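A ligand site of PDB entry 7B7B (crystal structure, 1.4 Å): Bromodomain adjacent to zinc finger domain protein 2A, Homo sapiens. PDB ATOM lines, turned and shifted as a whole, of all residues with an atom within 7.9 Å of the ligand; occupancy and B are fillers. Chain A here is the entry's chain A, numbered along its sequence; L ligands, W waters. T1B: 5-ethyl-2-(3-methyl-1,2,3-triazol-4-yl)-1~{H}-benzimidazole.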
ATOM      1  N   ALA A  22      15.756  -4.503  -8.351  1.00  0.00           N
ATOM      2  CA  ALA A  22      14.758  -4.756  -7.329  1.00  0.00           C
ATOM      3  C   ALA A  22      13.343  -4.872  -7.889  1.00  0.00           C
ATOM      4  O   ALA A  22      12.445  -5.297  -7.151  1.00  0.00           O
ATOM      5  CB  ALA A  22      14.787  -3.624  -6.307  1.00  0.00           C
ATOM      6  N   TRP A  23      13.115  -4.508  -9.148  1.00  0.00           N
ATOM      7  CA  TRP A  23      11.745  -4.428  -9.660  1.00  0.00           C
ATOM      8  C   TRP A  23      10.897  -5.677  -9.416  1.00  0.00           C
ATOM      9  O   TRP A  23       9.700  -5.524  -9.144  1.00  0.00           O
ATOM     10  CB  TRP A  23      11.739  -3.976 -11.145  1.00  0.00           C
ATOM     11  CG  TRP A  23      12.287  -4.991 -12.126  1.00  0.00           C
ATOM     12  CD1 TRP A  23      13.547  -5.048 -12.640  1.00  0.00           C
ATOM     13  CD2 TRP A  23      11.586  -6.120 -12.695  1.00  0.00           C
ATOM     14  NE1 TRP A  23      13.677  -6.129 -13.474  1.00  0.00           N
ATOM     15  CE2 TRP A  23      12.501  -6.809 -13.516  1.00  0.00           C
ATOM     16  CE3 TRP A  23      10.296  -6.614 -12.558  1.00  0.00           C
ATOM     17  CZ2 TRP A  23      12.137  -7.956 -14.237  1.00  0.00           C
ATOM     18  CZ3 TRP A  23       9.943  -7.752 -13.275  1.00  0.00           C
ATOM     19  CH2 TRP A  23      10.863  -8.404 -14.094  1.00  0.00           C
ATOM     20  N   PRO A  24      11.412  -6.903  -9.487  1.00  0.00           N
ATOM     21  CA  PRO A  24      10.537  -8.057  -9.265  1.00  0.00           C
ATOM     22  C   PRO A  24      10.080  -8.207  -7.834  1.00  0.00           C
ATOM     23  O   PRO A  24       9.129  -8.962  -7.590  1.00  0.00           O
ATOM     24  CB  PRO A  24      11.408  -9.260  -9.665  1.00  0.00           C
ATOM     25  CG  PRO A  24      12.491  -8.710 -10.489  1.00  0.00           C
ATOM     26  CD  PRO A  24      12.761  -7.340  -9.888  1.00  0.00           C
ATOM     27  N   PHE A  25      10.720  -7.483  -6.900  1.00  0.00           N
ATOM     28  CA  PHE A  25      10.589  -7.738  -5.466  1.00  0.00           C
ATOM     29  C   PHE A  25       9.993  -6.557  -4.723  1.00  0.00           C
ATOM     30  O   PHE A  25       9.896  -6.610  -3.491  1.00  0.00           O
ATOM     31  CB  PHE A  25      11.973  -8.090  -4.869  1.00  0.00           C
ATOM     32  CG  PHE A  25      12.745  -9.048  -5.718  1.00  0.00           C
ATOM     33  CD1 PHE A  25      12.261 -10.315  -5.936  1.00  0.00           C
ATOM     34  CD2 PHE A  25      13.911  -8.665  -6.314  1.00  0.00           C
ATOM     35  CE1 PHE A  25      12.932 -11.193  -6.755  1.00  0.00           C
ATOM     36  CE2 PHE A  25      14.605  -9.541  -7.149  1.00  0.00           C
ATOM     37  CZ  PHE A  25      14.104 -10.810  -7.368  1.00  0.00           C
ATOM     38  N   LEU A  26       9.584  -5.501  -5.426  1.00  0.00           N
ATOM     39  CA  LEU A  26       9.124  -4.288  -4.757  1.00  0.00           C
ATOM     40  C   LEU A  26       7.801  -4.509  -4.021  1.00  0.00           C
ATOM     41  O   LEU A  26       7.576  -3.939  -2.952  1.00  0.00           O
ATOM     42  CB  LEU A  26       8.956  -3.154  -5.770  1.00  0.00           C
ATOM     43  CG  LEU A  26      10.258  -2.696  -6.433  1.00  0.00           C
ATOM     44  CD1 LEU A  26       9.954  -1.590  -7.435  1.00  0.00           C
ATOM     45  CD2 LEU A  26      11.275  -2.249  -5.379  1.00  0.00           C
ATOM     46  N   GLU A  27       6.912  -5.302  -4.591  1.00  0.00           N
ATOM     47  CA  GLU A  27       5.592  -5.605  -4.039  1.00  0.00           C
ATOM     48  C   GLU A  27       5.390  -7.103  -4.068  1.00  0.00           C
ATOM     49  O   GLU A  27       6.145  -7.829  -4.714  1.00  0.00           O
ATOM     50  CB  GLU A  27       4.514  -4.924  -4.898  1.00  0.00           C
ATOM     51  CG  GLU A  27       4.580  -3.413  -4.877  1.00  0.00           C
ATOM     52  CD  GLU A  27       3.507  -2.804  -5.764  1.00  0.00           C
ATOM     53  OE1 GLU A  27       2.405  -2.559  -5.278  1.00  0.00           O
ATOM     54  OE2 GLU A  27       3.767  -2.602  -6.972  1.00  0.00           O
ATOM     55  N   PRO A  28       4.387  -7.603  -3.344  1.00  0.00           N
ATOM     56  CA  PRO A  28       4.130  -9.050  -3.343  1.00  0.00           C
ATOM     57  C   PRO A  28       4.026  -9.586  -4.768  1.00  0.00           C
ATOM     58  O   PRO A  28       3.513  -8.925  -5.676  1.00  0.00           O
ATOM     59  CB  PRO A  28       2.792  -9.173  -2.613  1.00  0.00           C
ATOM     60  CG  PRO A  28       2.723  -7.930  -1.750  1.00  0.00           C
ATOM     61  CD  PRO A  28       3.417  -6.859  -2.531  1.00  0.00           C
ATOM     62  N   VAL A  29       4.517 -10.803  -4.983  1.00  0.00           N
ATOM     63  CA  VAL A  29       4.309 -11.428  -6.286  1.00  0.00           C
ATOM     64  C   VAL A  29       2.821 -11.433  -6.571  1.00  0.00           C
ATOM     65  O   VAL A  29       2.024 -11.902  -5.759  1.00  0.00           O
ATOM     66  CB  VAL A  29       4.928 -12.831  -6.349  1.00  0.00           C
ATOM     67  CG1 VAL A  29       4.579 -13.487  -7.674  1.00  0.00           C
ATOM     68  CG2 VAL A  29       6.431 -12.725  -6.212  1.00  0.00           C
ATOM     69  N   ASN A  30       2.458 -10.926  -7.726  1.00  0.00           N
ATOM     70  CA  ASN A  30       1.096 -10.516  -7.994  1.00  0.00           C
ATOM     71  C   ASN A  30       0.415 -11.564  -8.858  1.00  0.00           C
ATOM     72  O   ASN A  30       0.822 -11.773 -10.012  1.00  0.00           O
ATOM     73  CB  ASN A  30       1.194  -9.194  -8.743  1.00  0.00           C
ATOM     74  CG  ASN A  30      -0.123  -8.549  -9.056  1.00  0.00           C
ATOM     75  OD1 ASN A  30      -1.193  -9.138  -8.942  1.00  0.00           O
ATOM     76  ND2 ASN A  30      -0.040  -7.298  -9.491  1.00  0.00           N
ATOM     77  N   LEU A  33      -0.233 -11.097 -12.530  1.00  0.00           N
ATOM     78  CA  LEU A  33       0.899 -11.097 -13.442  1.00  0.00           C
ATOM     79  C   LEU A  33       1.705 -12.395 -13.442  1.00  0.00           C
ATOM     80  O   LEU A  33       2.418 -12.658 -14.416  1.00  0.00           O
ATOM     81  CB  LEU A  33       1.857  -9.953 -13.073  1.00  0.00           C
ATOM     82  CG  LEU A  33       1.228  -8.560 -13.038  1.00  0.00           C
ATOM     83  CD1 LEU A  33       2.247  -7.511 -12.610  1.00  0.00           C
ATOM     84  CD2 LEU A  33       0.637  -8.223 -14.388  1.00  0.00           C
ATOM     85  N   VAL A  34       1.631 -13.193 -12.394  1.00  0.00           N
ATOM     86  CA  VAL A  34       2.459 -14.384 -12.232  1.00  0.00           C
ATOM     87  C   VAL A  34       1.559 -15.468 -11.711  1.00  0.00           C
ATOM     88  O   VAL A  34       0.969 -15.322 -10.630  1.00  0.00           O
ATOM     89  CB  VAL A  34       3.603 -14.142 -11.218  1.00  0.00           C
ATOM     90  CG1 VAL A  34       4.391 -15.410 -11.028  1.00  0.00           C
ATOM     91  CG2 VAL A  34       4.499 -12.997 -11.660  1.00  0.00           C
ATOM     92  N   SER A  35       1.470 -16.579 -12.442  1.00  0.00           N
ATOM     93  CA  SER A  35       0.583 -17.660 -12.040  1.00  0.00           C
ATOM     94  C   SER A  35       1.364 -18.740 -11.304  1.00  0.00           C
ATOM     95  O   SER A  35       2.573 -18.900 -11.485  1.00  0.00           O
ATOM     96  CB  SER A  35      -0.129 -18.253 -13.252  1.00  0.00           C
ATOM     97  OG  SER A  35       0.702 -19.154 -13.919  1.00  0.00           O
ATOM     98  N   TYR A  37       2.273 -19.094  -8.156  1.00  0.00           N
ATOM     99  CA  TYR A  37       3.368 -18.717  -7.277  1.00  0.00           C
ATOM    100  C   TYR A  37       3.200 -19.287  -5.863  1.00  0.00           C
ATOM    101  O   TYR A  37       4.039 -20.057  -5.388  1.00  0.00           O
ATOM    102  CB  TYR A  37       3.538 -17.203  -7.254  1.00  0.00           C
ATOM    103  CG  TYR A  37       4.779 -16.788  -6.493  1.00  0.00           C
ATOM    104  CD1 TYR A  37       6.043 -16.897  -7.072  1.00  0.00           C
ATOM    105  CD2 TYR A  37       4.706 -16.343  -5.165  1.00  0.00           C
ATOM    106  CE1 TYR A  37       7.191 -16.521  -6.364  1.00  0.00           C
ATOM    107  CE2 TYR A  37       5.841 -15.991  -4.467  1.00  0.00           C
ATOM    108  CZ  TYR A  37       7.081 -16.099  -5.068  1.00  0.00           C
ATOM    109  OH  TYR A  37       8.216 -15.747  -4.371  1.00  0.00           O
ATOM    110  N   ILE A  41       5.449 -21.455  -3.319  1.00  0.00           N
ATOM    111  CA  ILE A  41       6.164 -20.617  -2.357  1.00  0.00           C
ATOM    112  C   ILE A  41       5.264 -20.406  -1.151  1.00  0.00           C
ATOM    113  O   ILE A  41       4.272 -19.687  -1.220  1.00  0.00           O
ATOM    114  CB  ILE A  41       6.554 -19.264  -2.992  1.00  0.00           C
ATOM    115  CG1 ILE A  41       7.508 -19.486  -4.160  1.00  0.00           C
ATOM    116  CG2 ILE A  41       7.154 -18.332  -1.944  1.00  0.00           C
ATOM    117  CD1 ILE A  41       8.797 -20.169  -3.809  1.00  0.00           C
ATOM    118  N   MET A  45       7.564 -13.083   0.379  1.00  0.00           N
ATOM    119  CA  MET A  45       8.106 -11.876   1.006  1.00  0.00           C
ATOM    120  C   MET A  45       8.510 -10.913  -0.085  1.00  0.00           C
ATOM    121  O   MET A  45       8.893 -11.330  -1.176  1.00  0.00           O
ATOM    122  CB  MET A  45       9.271 -12.200   1.966  1.00  0.00           C
ATOM    123  CG  MET A  45       9.770 -11.032   2.799  1.00  0.00           C
ATOM    124  SD  MET A  45       8.497 -10.118   3.678  1.00  0.00           S
ATOM    125  CE  MET A  45       7.673 -11.440   4.565  1.00  0.00           C
ATOM    126  N   VAL A  72      13.205 -13.224   0.598  1.00  0.00           N
ATOM    127  CA  VAL A  72      12.990 -12.683  -0.748  1.00  0.00           C
ATOM    128  C   VAL A  72      13.872 -13.409  -1.759  1.00  0.00           C
ATOM    129  O   VAL A  72      13.398 -13.848  -2.816  1.00  0.00           O
ATOM    130  CB  VAL A  72      13.236 -11.161  -0.789  1.00  0.00           C
ATOM    131  CG1 VAL A  72      13.065 -10.661  -2.230  1.00  0.00           C
ATOM    132  CG2 VAL A  72      12.246 -10.443   0.114  1.00  0.00           C
ATOM    133  N   ASN A  75      13.140 -17.371  -1.983  1.00  0.00           N
ATOM    134  CA  ASN A  75      11.930 -17.653  -2.750  1.00  0.00           C
ATOM    135  C   ASN A  75      12.197 -17.479  -4.227  1.00  0.00           C
ATOM    136  O   ASN A  75      11.718 -18.264  -5.052  1.00  0.00           O
ATOM    137  CB  ASN A  75      10.810 -16.719  -2.331  1.00  0.00           C
ATOM    138  CG  ASN A  75      10.253 -17.046  -0.975  1.00  0.00           C
ATOM    139  OD1 ASN A  75      10.454 -18.139  -0.466  1.00  0.00           O
ATOM    140  ND2 ASN A  75       9.505 -16.108  -0.406  1.00  0.00           N
ATOM    141  N   CYS A  76      12.931 -16.427  -4.569  1.00  0.00           N
ATOM    142  CA  CYS A  76      13.223 -16.159  -5.969  1.00  0.00           C
ATOM    143  C   CYS A  76      14.001 -17.318  -6.594  1.00  0.00           C
ATOM    144  O   CYS A  76      13.700 -17.738  -7.710  1.00  0.00           O
ATOM    145  CB  CYS A  76      14.008 -14.855  -6.070  1.00  0.00           C
ATOM    146  SG  CYS A  76      14.406 -14.393  -7.768  1.00  0.00           S
ATOM    147  N   GLN A  77      14.987 -17.850  -5.893  1.00  0.00           N
ATOM    148  CA  GLN A  77      15.750 -18.952  -6.481  1.00  0.00           C
ATOM    149  C   GLN A  77      14.960 -20.254  -6.450  1.00  0.00           C
ATOM    150  O   GLN A  77      15.260 -21.155  -7.245  1.00  0.00           O
ATOM    151  CB  GLN A  77      17.121 -19.080  -5.803  1.00  0.00           C
ATOM    152  CG  GLN A  77      17.109 -19.669  -4.417  1.00  0.00           C
ATOM    153  CD  GLN A  77      18.503 -19.688  -3.773  1.00  0.00           C
ATOM    154  OE1 GLN A  77      19.500 -19.304  -4.388  1.00  0.00           O
ATOM    155  NE2 GLN A  77      18.564 -20.143  -2.508  1.00  0.00           N
ATOM    156  N   PHE A  79      11.597 -20.355  -7.157  1.00  0.00           N
ATOM    157  CA  PHE A  79      10.576 -20.271  -8.199  1.00  0.00           C
ATOM    158  C   PHE A  79      11.120 -20.077  -9.598  1.00  0.00           C
ATOM    159  O   PHE A  79      10.477 -20.495 -10.568  1.00  0.00           O
ATOM    160  CB  PHE A  79       9.658 -19.096  -7.895  1.00  0.00           C
ATOM    161  CG  PHE A  79       8.418 -19.085  -8.729  1.00  0.00           C
ATOM    162  CD1 PHE A  79       7.379 -19.946  -8.444  1.00  0.00           C
ATOM    163  CD2 PHE A  79       8.286 -18.199  -9.798  1.00  0.00           C
ATOM    164  CE1 PHE A  79       6.216 -19.940  -9.206  1.00  0.00           C
ATOM    165  CE2 PHE A  79       7.119 -18.209 -10.567  1.00  0.00           C
ATOM    166  CZ  PHE A  79       6.095 -19.089 -10.277  1.00  0.00           C
ATOM    167  N   ASN A  80      12.272 -19.419  -9.731  1.00  0.00           N
ATOM    168  CA  ASN A  80      12.752 -18.942 -11.023  1.00  0.00           C
ATOM    169  C   ASN A  80      14.023 -19.657 -11.423  1.00  0.00           C
ATOM    170  O   ASN A  80      14.879 -19.937 -10.578  1.00  0.00           O
ATOM    171  CB  ASN A  80      13.023 -17.440 -10.981  1.00  0.00           C
ATOM    172  CG  ASN A  80      11.793 -16.650 -10.634  1.00  0.00           C
ATOM    173  OD1 ASN A  80      10.948 -16.404 -11.481  1.00  0.00           O
ATOM    174  ND2 ASN A  80      11.693 -16.250  -9.390  1.00  0.00           N
ATOM    175  N   SER A  84      16.826 -16.893 -15.872  1.00  0.00           N
ATOM    176  CA  SER A  84      15.707 -16.030 -16.185  1.00  0.00           C
ATOM    177  C   SER A  84      15.998 -14.606 -15.693  1.00  0.00           C
ATOM    178  O   SER A  84      16.861 -14.383 -14.851  1.00  0.00           O
ATOM    179  CB  SER A  84      14.436 -16.533 -15.523  1.00  0.00           C
ATOM    180  OG  SER A  84      14.503 -16.378 -14.120  1.00  0.00           O
ATOM    181  N   VAL A  86      14.134 -12.668 -13.817  1.00  0.00           N
ATOM    182  CA  VAL A  86      13.869 -12.521 -12.395  1.00  0.00           C
ATOM    183  C   VAL A  86      14.881 -13.301 -11.573  1.00  0.00           C
ATOM    184  O   VAL A  86      15.346 -12.836 -10.526  1.00  0.00           O
ATOM    185  CB  VAL A  86      12.408 -12.911 -12.098  1.00  0.00           C
ATOM    186  CG1 VAL A  86      12.171 -12.985 -10.598  1.00  0.00           C
ATOM    187  CG2 VAL A  86      11.483 -11.891 -12.727  1.00  0.00           C
ATOM    188  N   GLY A  87      15.293 -14.482 -12.057  1.00  0.00           N
ATOM    189  CA  GLY A  87      16.313 -15.224 -11.343  1.00  0.00           C
ATOM    190  C   GLY A  87      17.626 -14.453 -11.226  1.00  0.00           C
ATOM    191  O   GLY A  87      18.235 -14.416 -10.157  1.00  0.00           O
HETATM  192  C12 T1B L   1       8.631 -12.453  -9.646  1.00  0.00           C
HETATM  193  C13 T1B L   1       9.172 -12.330  -8.387  1.00  0.00           C
HETATM  194  C01 T1B L   1       4.979  -5.543 -11.116  1.00  0.00           C
HETATM  195  C02 T1B L   1       5.958  -5.993 -12.202  1.00  0.00           C
HETATM  196  C03 T1B L   1       6.337  -7.478 -12.139  1.00  0.00           C
HETATM  197  C04 T1B L   1       6.069  -8.357 -13.200  1.00  0.00           C
HETATM  198  C05 T1B L   1       6.429  -9.686 -13.113  1.00  0.00           C
HETATM  199  C06 T1B L   1       7.060 -10.156 -11.951  1.00  0.00           C
HETATM  200  C08 T1B L   1       8.034 -11.318 -10.430  1.00  0.00           C
HETATM  201  C10 T1B L   1       7.335  -9.314 -10.924  1.00  0.00           C
HETATM  202  C11 T1B L   1       6.965  -7.957 -10.997  1.00  0.00           C
HETATM  203  C17 T1B L   1       8.245 -14.389 -11.171  1.00  0.00           C
HETATM  204  N07 T1B L   1       7.496 -11.387 -11.639  1.00  0.00           N
HETATM  205  N09 T1B L   1       7.931 -10.053  -9.973  1.00  0.00           N
HETATM  206  N14 T1B L   1       9.576 -13.512  -8.000  1.00  0.00           N
HETATM  207  N15 T1B L   1       9.248 -14.396  -8.972  1.00  0.00           N
HETATM  208  N16 T1B L   1       8.677 -13.728  -9.976  1.00  0.00           N
HETATM  209  O   HOH W   1       4.433  -9.756  -9.499  1.00  0.00           O
HETATM  210  O   HOH W   2       7.484 -12.888 -14.256  1.00  0.00           O
HETATM  211  O   HOH W   3      10.212 -14.874  -5.755  1.00  0.00           O
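O of Pro 24 lies close to N09 of the ligand, 2.9 Å away.
The side-chain amide nitrogen (ND2) of Asn 80 lies within hydrogen-bond range of a nitrogen (N15) of the ligand (3.1 Å).
The side-chain amide nitrogen (ND2) of Asn 80 sits at hydrogen-bond distance from the backbone carbonyl oxygen (O) of Cys 76 (3.0 Å).
The side-chain sulfur (SG) of Cys 76 is in hydrogen-bond range of the backbone carbonyl oxygen (O) of Val 86 (3.3 Å).
Trp 23 touches the ligand.
CG2 of Val 29 touches C13 of the ligand, 3.5 Å away.
Leu 33 touches the ligand (CD1 to C01, 3.7 Å).
Val 34 touches the ligand (CG2 to N07, 3.4 Å).
Tyr 37 touches the ligand (CE1 to N15, 3.9 Å).
CG1 of Val 86 touches N16 of the ligand (3.6 Å).
Hydrophobic or aromatic side chains that line the ligand: Trp 23, Pro 24, Val 29, Leu 33, Val 34, Tyr 37 and Val 86.
The nearest printed residue that does not touch the ligand is Phe 79 (4.01 Å).
Water W3 lies within hydrogen-bond range of the side-chain hydroxyl of Tyr 37 (2.6 Å), a nitrogen (N14) of the ligand (2.7 Å) and the backbone NH of Cys 76 (3.3 Å).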
